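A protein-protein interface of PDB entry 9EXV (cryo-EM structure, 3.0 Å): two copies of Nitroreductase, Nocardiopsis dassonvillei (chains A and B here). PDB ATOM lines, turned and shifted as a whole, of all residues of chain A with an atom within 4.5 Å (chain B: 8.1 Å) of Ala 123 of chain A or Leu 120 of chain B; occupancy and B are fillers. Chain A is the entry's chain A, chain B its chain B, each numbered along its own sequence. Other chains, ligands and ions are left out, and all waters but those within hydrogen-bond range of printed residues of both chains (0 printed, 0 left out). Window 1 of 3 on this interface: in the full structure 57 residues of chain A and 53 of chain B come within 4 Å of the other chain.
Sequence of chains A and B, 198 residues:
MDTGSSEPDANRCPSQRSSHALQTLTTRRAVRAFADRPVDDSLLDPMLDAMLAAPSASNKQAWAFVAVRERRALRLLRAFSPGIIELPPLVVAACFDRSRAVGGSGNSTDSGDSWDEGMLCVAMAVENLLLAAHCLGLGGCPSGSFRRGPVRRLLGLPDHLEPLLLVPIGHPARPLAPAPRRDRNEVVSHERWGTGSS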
ATOM      1  N   TRP A 115     -36.829 -23.327  -9.370  1.00  0.00           N
ATOM      2  CA  TRP A 115     -36.577 -21.893  -9.306  1.00  0.00           C
ATOM      3  C   TRP A 115     -37.886 -21.113  -9.282  1.00  0.00           C
ATOM      4  O   TRP A 115     -38.862 -21.499  -9.927  1.00  0.00           O
ATOM      5  CB  TRP A 115     -35.718 -21.447 -10.489  1.00  0.00           C
ATOM      6  CG  TRP A 115     -35.441 -19.977 -10.500  1.00  0.00           C
ATOM      7  CD1 TRP A 115     -36.113 -19.021 -11.203  1.00  0.00           C
ATOM      8  CD2 TRP A 115     -34.420 -19.293  -9.765  1.00  0.00           C
ATOM      9  NE1 TRP A 115     -35.571 -17.783 -10.954  1.00  0.00           N
ATOM     10  CE2 TRP A 115     -34.531 -17.923 -10.074  1.00  0.00           C
ATOM     11  CE3 TRP A 115     -33.422 -19.705  -8.877  1.00  0.00           C
ATOM     12  CZ2 TRP A 115     -33.683 -16.966  -9.527  1.00  0.00           C
ATOM     13  CZ3 TRP A 115     -32.581 -18.751  -8.335  1.00  0.00           C
ATOM     14  CH2 TRP A 115     -32.717 -17.399  -8.663  1.00  0.00           C
ATOM     15  N   MET A 119     -37.632 -15.326  -5.665  1.00  0.00           N
ATOM     16  CA  MET A 119     -36.236 -15.321  -5.244  1.00  0.00           C
ATOM     17  C   MET A 119     -35.505 -14.109  -5.803  1.00  0.00           C
ATOM     18  O   MET A 119     -34.685 -13.489  -5.116  1.00  0.00           O
ATOM     19  CB  MET A 119     -35.559 -16.622  -5.682  1.00  0.00           C
ATOM     20  CG  MET A 119     -36.068 -17.861  -4.952  1.00  0.00           C
ATOM     21  SD  MET A 119     -35.597 -19.426  -5.723  1.00  0.00           S
ATOM     22  CE  MET A 119     -34.044 -19.782  -4.910  1.00  0.00           C
ATOM     23  N   LEU A 120     -35.809 -13.744  -7.049  1.00  0.00           N
ATOM     24  CA  LEU A 120     -35.235 -12.535  -7.622  1.00  0.00           C
ATOM     25  C   LEU A 120     -35.669 -11.299  -6.843  1.00  0.00           C
ATOM     26  O   LEU A 120     -34.890 -10.351  -6.696  1.00  0.00           O
ATOM     27  CB  LEU A 120     -35.625 -12.415  -9.094  1.00  0.00           C
ATOM     28  CG  LEU A 120     -35.123 -13.541 -10.000  1.00  0.00           C
ATOM     29  CD1 LEU A 120     -35.684 -13.389 -11.401  1.00  0.00           C
ATOM     30  CD2 LEU A 120     -33.603 -13.574 -10.035  1.00  0.00           C
ATOM     31  N   CYS A 121     -36.903 -11.288  -6.338  1.00  0.00           N
ATOM     32  CA  CYS A 121     -37.345 -10.164  -5.515  1.00  0.00           C
ATOM     33  C   CYS A 121     -36.578 -10.106  -4.199  1.00  0.00           C
ATOM     34  O   CYS A 121     -36.279  -9.018  -3.696  1.00  0.00           O
ATOM     35  CB  CYS A 121     -38.848 -10.253  -5.262  1.00  0.00           C
ATOM     36  SG  CYS A 121     -39.860  -9.984  -6.735  1.00  0.00           S
ATOM     37  N   VAL A 122     -36.262 -11.267  -3.621  1.00  0.00           N
ATOM     38  CA  VAL A 122     -35.384 -11.302  -2.458  1.00  0.00           C
ATOM     39  C   VAL A 122     -34.052 -10.642  -2.793  1.00  0.00           C
ATOM     40  O   VAL A 122     -33.540  -9.806  -2.040  1.00  0.00           O
ATOM     41  CB  VAL A 122     -35.193 -12.751  -1.975  1.00  0.00           C
ATOM     42  CG1 VAL A 122     -34.334 -12.798  -0.720  1.00  0.00           C
ATOM     43  CG2 VAL A 122     -36.539 -13.424  -1.734  1.00  0.00           C
ATOM     44  N   ALA A 123     -33.487 -10.985  -3.951  1.00  0.00           N
ATOM     45  CA  ALA A 123     -32.234 -10.379  -4.378  1.00  0.00           C
ATOM     46  C   ALA A 123     -32.381  -8.875  -4.583  1.00  0.00           C
ATOM     47  O   ALA A 123     -31.455  -8.109  -4.293  1.00  0.00           O
ATOM     48  CB  ALA A 123     -31.739 -11.051  -5.660  1.00  0.00           C
ATOM     49  N   MET A 124     -33.530  -8.435  -5.104  1.00  0.00           N
ATOM     50  CA  MET A 124     -33.758  -7.007  -5.308  1.00  0.00           C
ATOM     51  C   MET A 124     -33.790  -6.259  -3.983  1.00  0.00           C
ATOM     52  O   MET A 124     -33.216  -5.172  -3.857  1.00  0.00           O
ATOM     53  CB  MET A 124     -35.062  -6.796  -6.077  1.00  0.00           C
ATOM     54  CG  MET A 124     -35.049  -7.340  -7.501  1.00  0.00           C
ATOM     55  SD  MET A 124     -36.652  -7.212  -8.316  1.00  0.00           S
ATOM     56  CE  MET A 124     -36.354  -8.100  -9.842  1.00  0.00           C
ATOM     57  N   ALA A 125     -34.470  -6.824  -2.983  1.00  0.00           N
ATOM     58  CA  ALA A 125     -34.431  -6.237  -1.654  1.00  0.00           C
ATOM     59  C   ALA A 125     -33.012  -6.203  -1.110  1.00  0.00           C
ATOM     60  O   ALA A 125     -32.644  -5.264  -0.398  1.00  0.00           O
ATOM     61  CB  ALA A 125     -35.356  -7.001  -0.706  1.00  0.00           C
ATOM     62  N   VAL A 126     -32.195  -7.200  -1.447  1.00  0.00           N
ATOM     63  CA  VAL A 126     -30.799  -7.172  -1.030  1.00  0.00           C
ATOM     64  C   VAL A 126     -30.052  -6.031  -1.715  1.00  0.00           C
ATOM     65  O   VAL A 126     -29.169  -5.408  -1.120  1.00  0.00           O
ATOM     66  CB  VAL A 126     -30.132  -8.532  -1.296  1.00  0.00           C
ATOM     67  CG1 VAL A 126     -28.623  -8.407  -1.205  1.00  0.00           C
ATOM     68  CG2 VAL A 126     -30.644  -9.565  -0.305  1.00  0.00           C
ATOM     69  N   GLU A 127     -30.375  -5.743  -2.978  1.00  0.00           N
ATOM     70  CA  GLU A 127     -29.767  -4.592  -3.637  1.00  0.00           C
ATOM     71  C   GLU A 127     -30.122  -3.304  -2.912  1.00  0.00           C
ATOM     72  O   GLU A 127     -29.261  -2.455  -2.660  1.00  0.00           O
ATOM     73  CB  GLU A 127     -30.216  -4.514  -5.095  1.00  0.00           C
ATOM     74  CG  GLU A 127     -29.654  -3.308  -5.826  1.00  0.00           C
ATOM     75  CD  GLU A 127     -28.142  -3.254  -5.750  1.00  0.00           C
ATOM     76  OE1 GLU A 127     -27.497  -4.289  -6.017  1.00  0.00           O
ATOM     77  OE2 GLU A 127     -27.596  -2.184  -5.407  1.00  0.00           O
ATOM     78  N   LEU A 165     -29.248 -15.259   0.582  1.00  0.00           N
ATOM     79  CA  LEU A 165     -28.092 -14.383   0.663  1.00  0.00           C
ATOM     80  C   LEU A 165     -27.777 -14.094   2.120  1.00  0.00           C
ATOM     81  O   LEU A 165     -28.656 -14.136   2.984  1.00  0.00           O
ATOM     82  CB  LEU A 165     -28.327 -13.077  -0.110  1.00  0.00           C
ATOM     83  CG  LEU A 165     -28.342 -13.233  -1.632  1.00  0.00           C
ATOM     84  CD1 LEU A 165     -28.987 -12.037  -2.309  1.00  0.00           C
ATOM     85  CD2 LEU A 165     -26.929 -13.439  -2.152  1.00  0.00           C
ATOM     86  N   ALA B  54     -23.596  -2.555 -10.851  1.00  0.00           N
ATOM     87  CA  ALA B  54     -24.239  -3.476  -9.930  1.00  0.00           C
ATOM     88  C   ALA B  54     -23.315  -4.646  -9.633  1.00  0.00           C
ATOM     89  O   ALA B  54     -22.490  -5.019 -10.473  1.00  0.00           O
ATOM     90  CB  ALA B  54     -25.561  -4.001 -10.504  1.00  0.00           C
ATOM     91  N   PRO B  55     -23.431  -5.243  -8.449  1.00  0.00           N
ATOM     92  CA  PRO B  55     -22.575  -6.383  -8.120  1.00  0.00           C
ATOM     93  C   PRO B  55     -22.877  -7.588  -8.995  1.00  0.00           C
ATOM     94  O   PRO B  55     -24.007  -7.801  -9.439  1.00  0.00           O
ATOM     95  CB  PRO B  55     -22.908  -6.667  -6.648  1.00  0.00           C
ATOM     96  CG  PRO B  55     -24.267  -6.098  -6.451  1.00  0.00           C
ATOM     97  CD  PRO B  55     -24.344  -4.896  -7.344  1.00  0.00           C
ATOM     98  N   SER B  56     -21.838  -8.376  -9.243  1.00  0.00           N
ATOM     99  CA  SER B  56     -21.904  -9.589 -10.043  1.00  0.00           C
ATOM    100  C   SER B  56     -21.502 -10.778  -9.179  1.00  0.00           C
ATOM    101  O   SER B  56     -21.213 -10.636  -7.994  1.00  0.00           O
ATOM    102  CB  SER B  56     -21.003  -9.478 -11.273  1.00  0.00           C
ATOM    103  OG  SER B  56     -19.644  -9.555 -10.909  1.00  0.00           O
ATOM    104  N   ALA B  57     -21.489 -11.967  -9.782  1.00  0.00           N
ATOM    105  CA  ALA B  57     -21.062 -13.148  -9.039  1.00  0.00           C
ATOM    106  C   ALA B  57     -19.580 -13.073  -8.689  1.00  0.00           C
ATOM    107  O   ALA B  57     -19.202 -13.192  -7.518  1.00  0.00           O
ATOM    108  CB  ALA B  57     -21.366 -14.414  -9.840  1.00  0.00           C
ATOM    109  N   ALA B  62     -21.497 -11.303 -15.760  1.00  0.00           N
ATOM    110  CA  ALA B  62     -22.215 -12.352 -16.480  1.00  0.00           C
ATOM    111  C   ALA B  62     -23.681 -11.951 -16.619  1.00  0.00           C
ATOM    112  O   ALA B  62     -24.560 -12.403 -15.880  1.00  0.00           O
ATOM    113  CB  ALA B  62     -22.067 -13.687 -15.765  1.00  0.00           C
ATOM    114  N   TRP B  63     -23.946 -11.082 -17.591  1.00  0.00           N
ATOM    115  CA  TRP B  63     -25.311 -10.684 -17.901  1.00  0.00           C
ATOM    116  C   TRP B  63     -25.342 -10.034 -19.275  1.00  0.00           C
ATOM    117  O   TRP B  63     -24.305  -9.717 -19.864  1.00  0.00           O
ATOM    118  CB  TRP B  63     -25.880  -9.737 -16.844  1.00  0.00           C
ATOM    119  CG  TRP B  63     -25.107  -8.473 -16.689  1.00  0.00           C
ATOM    120  CD1 TRP B  63     -25.098  -7.410 -17.536  1.00  0.00           C
ATOM    121  CD2 TRP B  63     -24.234  -8.133 -15.611  1.00  0.00           C
ATOM    122  NE1 TRP B  63     -24.275  -6.424 -17.051  1.00  0.00           N
ATOM    123  CE2 TRP B  63     -23.727  -6.846 -15.872  1.00  0.00           C
ATOM    124  CE3 TRP B  63     -23.827  -8.795 -14.452  1.00  0.00           C
ATOM    125  CZ2 TRP B  63     -22.836  -6.208 -15.017  1.00  0.00           C
ATOM    126  CZ3 TRP B  63     -22.950  -8.161 -13.606  1.00  0.00           C
ATOM    127  CH2 TRP B  63     -22.459  -6.883 -13.891  1.00  0.00           C
ATOM    128  N   PHE B  96     -29.469 -13.669 -18.318  1.00  0.00           N
ATOM    129  CA  PHE B  96     -28.327 -14.298 -17.671  1.00  0.00           C
ATOM    130  C   PHE B  96     -27.373 -14.822 -18.734  1.00  0.00           C
ATOM    131  O   PHE B  96     -27.800 -15.453 -19.706  1.00  0.00           O
ATOM    132  CB  PHE B  96     -28.754 -15.433 -16.743  1.00  0.00           C
ATOM    133  CG  PHE B  96     -27.611 -16.034 -15.976  1.00  0.00           C
ATOM    134  CD1 PHE B  96     -26.670 -15.214 -15.377  1.00  0.00           C
ATOM    135  CD2 PHE B  96     -27.472 -17.406 -15.855  1.00  0.00           C
ATOM    136  CE1 PHE B  96     -25.610 -15.747 -14.673  1.00  0.00           C
ATOM    137  CE2 PHE B  96     -26.414 -17.945 -15.148  1.00  0.00           C
ATOM    138  CZ  PHE B  96     -25.481 -17.113 -14.556  1.00  0.00           C
ATOM    139  N   TRP B 115     -31.231 -22.115 -12.313  1.00  0.00           N
ATOM    140  CA  TRP B 115     -30.669 -22.412 -11.002  1.00  0.00           C
ATOM    141  C   TRP B 115     -29.202 -21.985 -10.932  1.00  0.00           C
ATOM    142  O   TRP B 115     -28.296 -22.810 -10.978  1.00  0.00           O
ATOM    143  CB  TRP B 115     -30.815 -23.905 -10.683  1.00  0.00           C
ATOM    144  CG  TRP B 115     -30.191 -24.823 -11.706  1.00  0.00           C
ATOM    145  CD1 TRP B 115     -28.932 -25.355 -11.676  1.00  0.00           C
ATOM    146  CD2 TRP B 115     -30.800 -25.317 -12.906  1.00  0.00           C
ATOM    147  NE1 TRP B 115     -28.717 -26.135 -12.778  1.00  0.00           N
ATOM    148  CE2 TRP B 115     -29.848 -26.134 -13.549  1.00  0.00           C
ATOM    149  CE3 TRP B 115     -32.055 -25.149 -13.497  1.00  0.00           C
ATOM    150  CZ2 TRP B 115     -30.113 -26.781 -14.754  1.00  0.00           C
ATOM    151  CZ3 TRP B 115     -32.315 -25.793 -14.695  1.00  0.00           C
ATOM    152  CH2 TRP B 115     -31.349 -26.598 -15.309  1.00  0.00           C
ATOM    153  N   ASP B 116     -28.964 -20.682 -10.819  1.00  0.00           N
ATOM    154  CA  ASP B 116     -27.605 -20.162 -10.792  1.00  0.00           C
ATOM    155  C   ASP B 116     -27.524 -19.000  -9.814  1.00  0.00           C
ATOM    156  O   ASP B 116     -28.413 -18.146  -9.777  1.00  0.00           O
ATOM    157  CB  ASP B 116     -27.154 -19.715 -12.188  1.00  0.00           C
ATOM    158  CG  ASP B 116     -25.645 -19.652 -12.322  1.00  0.00           C
ATOM    159  OD1 ASP B 116     -24.977 -19.195 -11.373  1.00  0.00           O
ATOM    160  OD2 ASP B 116     -25.126 -20.069 -13.379  1.00  0.00           O
ATOM    161  N   GLU B 117     -26.448 -18.978  -9.024  1.00  0.00           N
ATOM    162  CA  GLU B 117     -26.248 -17.893  -8.071  1.00  0.00           C
ATOM    163  C   GLU B 117     -26.148 -16.548  -8.777  1.00  0.00           C
ATOM    164  O   GLU B 117     -26.761 -15.564  -8.346  1.00  0.00           O
ATOM    165  CB  GLU B 117     -24.994 -18.159  -7.239  1.00  0.00           C
ATOM    166  CG  GLU B 117     -24.401 -16.937  -6.555  1.00  0.00           C
ATOM    167  CD  GLU B 117     -23.109 -17.245  -5.823  1.00  0.00           C
ATOM    168  OE1 GLU B 117     -22.895 -18.424  -5.472  1.00  0.00           O
ATOM    169  OE2 GLU B 117     -22.305 -16.316  -5.609  1.00  0.00           O
ATOM    170  N   GLY B 118     -25.387 -16.489  -9.871  1.00  0.00           N
ATOM    171  CA  GLY B 118     -25.213 -15.240 -10.587  1.00  0.00           C
ATOM    172  C   GLY B 118     -26.491 -14.687 -11.179  1.00  0.00           C
ATOM    173  O   GLY B 118     -26.561 -13.489 -11.470  1.00  0.00           O
ATOM    174  N   MET B 119     -27.506 -15.534 -11.361  1.00  0.00           N
ATOM    175  CA  MET B 119     -28.781 -15.058 -11.885  1.00  0.00           C
ATOM    176  C   MET B 119     -29.407 -14.015 -10.964  1.00  0.00           C
ATOM    177  O   MET B 119     -30.174 -13.162 -11.425  1.00  0.00           O
ATOM    178  CB  MET B 119     -29.730 -16.239 -12.094  1.00  0.00           C
ATOM    179  CG  MET B 119     -31.035 -15.883 -12.783  1.00  0.00           C
ATOM    180  SD  MET B 119     -32.104 -17.312 -13.051  1.00  0.00           S
ATOM    181  CE  MET B 119     -31.213 -18.179 -14.342  1.00  0.00           C
ATOM    182  N   LEU B 120     -29.095 -14.067  -9.667  1.00  0.00           N
ATOM    183  CA  LEU B 120     -29.583 -13.056  -8.736  1.00  0.00           C
ATOM    184  C   LEU B 120     -28.941 -11.696  -8.986  1.00  0.00           C
ATOM    185  O   LEU B 120     -29.588 -10.659  -8.795  1.00  0.00           O
ATOM    186  CB  LEU B 120     -29.328 -13.500  -7.295  1.00  0.00           C
ATOM    187  CG  LEU B 120     -30.091 -14.720  -6.773  1.00  0.00           C
ATOM    188  CD1 LEU B 120     -29.850 -14.901  -5.282  1.00  0.00           C
ATOM    189  CD2 LEU B 120     -31.575 -14.596  -7.063  1.00  0.00           C
ATOM    190  N   CYS B 121     -27.672 -11.679  -9.394  1.00  0.00           N
ATOM    191  CA  CYS B 121     -26.980 -10.417  -9.623  1.00  0.00           C
ATOM    192  C   CYS B 121     -27.617  -9.622 -10.755  1.00  0.00           C
ATOM    193  O   CYS B 121     -27.639  -8.388 -10.713  1.00  0.00           O
ATOM    194  CB  CYS B 121     -25.504 -10.681  -9.912  1.00  0.00           C
ATOM    195  SG  CYS B 121     -24.633 -11.508  -8.563  1.00  0.00           S
ATOM    196  N   VAL B 122     -28.129 -10.309 -11.777  1.00  0.00           N
ATOM    197  CA  VAL B 122     -28.820  -9.618 -12.862  1.00  0.00           C
ATOM    198  C   VAL B 122     -30.063  -8.912 -12.336  1.00  0.00           C
ATOM    199  O   VAL B 122     -30.354  -7.770 -12.713  1.00  0.00           O
ATOM    200  CB  VAL B 122     -29.152 -10.611 -13.990  1.00  0.00           C
ATOM    201  CG1 VAL B 122     -29.822  -9.895 -15.149  1.00  0.00           C
ATOM    202  CG2 VAL B 122     -27.890 -11.330 -14.447  1.00  0.00           C
ATOM    203  N   ALA B 123     -30.815  -9.578 -11.459  1.00  0.00           N
ATOM    204  CA  ALA B 123     -31.970  -8.939 -10.843  1.00  0.00           C
ATOM    205  C   ALA B 123     -31.548  -7.762  -9.971  1.00  0.00           C
ATOM    206  O   ALA B 123     -32.263  -6.757  -9.882  1.00  0.00           O
ATOM    207  CB  ALA B 123     -32.763  -9.956 -10.026  1.00  0.00           C
ATOM    208  N   MET B 124     -30.394  -7.870  -9.309  1.00  0.00           N
ATOM    209  CA  MET B 124     -29.867  -6.733  -8.565  1.00  0.00           C
ATOM    210  C   MET B 124     -29.606  -5.550  -9.486  1.00  0.00           C
ATOM    211  O   MET B 124     -29.925  -4.403  -9.147  1.00  0.00           O
ATOM    212  CB  MET B 124     -28.584  -7.131  -7.833  1.00  0.00           C
ATOM    213  CG  MET B 124     -28.815  -7.849  -6.518  1.00  0.00           C
ATOM    214  SD  MET B 124     -27.286  -8.422  -5.759  1.00  0.00           S
ATOM    215  CE  MET B 124     -27.777 -10.071  -5.271  1.00  0.00           C
ATOM    216  N   ALA B 125     -29.027  -5.810 -10.660  1.00  0.00           N
ATOM    217  CA  ALA B 125     -28.821  -4.749 -11.637  1.00  0.00           C
ATOM    218  C   ALA B 125     -30.144  -4.141 -12.076  1.00  0.00           C
ATOM    219  O   ALA B 125     -30.251  -2.921 -12.242  1.00  0.00           O
ATOM    220  CB  ALA B 125     -28.050  -5.292 -12.842  1.00  0.00           C
ATOM    221  N   VAL B 126     -31.164  -4.978 -12.272  1.00  0.00           N
ATOM    222  CA  VAL B 126     -32.481  -4.470 -12.634  1.00  0.00           C
ATOM    223  C   VAL B 126     -33.023  -3.558 -11.541  1.00  0.00           C
ATOM    224  O   VAL B 126     -33.611  -2.506 -11.824  1.00  0.00           O
ATOM    225  CB  VAL B 126     -33.444  -5.637 -12.923  1.00  0.00           C
ATOM    226  CG1 VAL B 126     -34.864  -5.125 -13.055  1.00  0.00           C
ATOM    227  CG2 VAL B 126     -33.015  -6.376 -14.181  1.00  0.00           C
ATOM    228  N   GLU B 127     -32.845  -3.949 -10.277  1.00  0.00           N
ATOM    229  CA  GLU B 127     -33.265  -3.100  -9.169  1.00  0.00           C
ATOM    230  C   GLU B 127     -32.556  -1.755  -9.207  1.00  0.00           C
ATOM    231  O   GLU B 127     -33.176  -0.708  -8.990  1.00  0.00           O
ATOM    232  CB  GLU B 127     -32.989  -3.805  -7.840  1.00  0.00           C
ATOM    233  CG  GLU B 127     -33.294  -2.964  -6.623  1.00  0.00           C
ATOM    234  CD  GLU B 127     -34.740  -2.508  -6.581  1.00  0.00           C
ATOM    235  OE1 GLU B 127     -35.619  -3.294  -6.986  1.00  0.00           O
ATOM    236  OE2 GLU B 127     -34.996  -1.365  -6.149  1.00  0.00           O
ATOM    237  N   LEU B 164     -34.634 -13.172 -18.539  1.00  0.00           N
ATOM    238  CA  LEU B 164     -35.232 -13.427 -17.236  1.00  0.00           C
ATOM    239  C   LEU B 164     -36.064 -12.272 -16.695  1.00  0.00           C
ATOM    240  O   LEU B 164     -36.903 -12.508 -15.819  1.00  0.00           O
ATOM    241  CB  LEU B 164     -34.146 -13.785 -16.207  1.00  0.00           C
ATOM    242  CG  LEU B 164     -33.121 -12.709 -15.831  1.00  0.00           C
ATOM    243  CD1 LEU B 164     -33.605 -11.856 -14.675  1.00  0.00           C
ATOM    244  CD2 LEU B 164     -31.783 -13.332 -15.480  1.00  0.00           C
ATOM    245  N   LEU B 165     -35.857 -11.042 -17.164  1.00  0.00           N
ATOM    246  CA  LEU B 165     -36.609  -9.890 -16.682  1.00  0.00           C
ATOM    247  C   LEU B 165     -36.855  -8.916 -17.821  1.00  0.00           C
ATOM    248  O   LEU B 165     -35.937  -8.607 -18.587  1.00  0.00           O
ATOM    249  CB  LEU B 165     -35.872  -9.179 -15.540  1.00  0.00           C
ATOM    250  CG  LEU B 165     -36.215  -9.623 -14.117  1.00  0.00           C
ATOM    251  CD1 LEU B 165     -35.229  -9.034 -13.120  1.00  0.00           C
ATOM    252  CD2 LEU B 165     -37.636  -9.230 -13.758  1.00  0.00           C
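Printed residues of chain B that touch a printed residue of chain A: Pro 55, Met 119, Leu 120, Ala 123, Met 124, Glu 127 and Leu 165. Printed residues of chain A that touch a printed residue of chain B: Trp 115, Met 119, Leu 120, Ala 123, Met 124, Glu 127 and Leu 165. Along chain A the printed residues that touch a printed residue of chain B span positions 115 to 165. Among the printed residues, 15 pairs touch across the chains.
Ala 123 of chain A touches just these residues of chain B: Leu 120 (3.8 Å) and Met 124 (3.5 Å). Leu 120 of chain B touches four residues of chain A. Of the printed residues of chain B, Leu 120 of chain A touches Met 119 (3.7 Å), Leu 120 (3.7 Å) and Ala 123 (3.7 Å). Printed residues of chain A within 4 Å of Met 124 of chain B: Ala 123 (3.5 Å), Glu 127 (3.5 Å) and Leu 165 (3.8 Å). Of the printed residues of chain A, Leu 165 of chain B touches Met 124 (3.6 Å). Of the printed residues of chain A, Ala 123 of chain B touches Leu 120 and Met 124. Of the printed residues of chain A, Pro 55 of chain B touches Glu 127 (3.5 Å). The nearest residue of chain A that does not touch Leu 120 of chain B is Leu 165 of chain A (4.2 Å).
Trp 115 of chain A touches Leu 120 of chain B, but with the chains exchanged Leu 120 of chain A does not touch Trp 115 of chain B (9.2 Å). Leu 120 of chain B touches its own counterpart, Leu 120 of chain A. Ala 123 of chain A touches Met 124 of chain B, and with the chains exchanged Met 124 of chain A touches Ala 123 of chain B. Glu 127 of chain A touches its own counterpart, Glu 127 of chain B. 11 positions are printed for both chains.
Met 119 of chain B touches Trp 115 of chain A (SD to CZ2, 3.9 Å). Trp 115 of chain A touches Leu 120 of chain B (CH2 to CD2, 3.4 Å). Met 119 of chain A touches Leu 120 of chain B. Leu 120 of chain A touches Leu 120 of chain B. Leu 120 of chain A touches Ala 123 of chain B (CD2 to CB, 3.7 Å). CB of Ala 123 of chain A touches CB of Leu 120 of chain B, 3.8 Å away. Met 124 of chain A touches Ala 123 of chain B. Met 124 of chain A touches Glu 127 of chain B (O to CG, 3.5 Å). Met 124 of chain A touches Leu 165 of chain B. Glu 127 of chain A touches Met 124 of chain B (CG to O, 3.5 Å).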
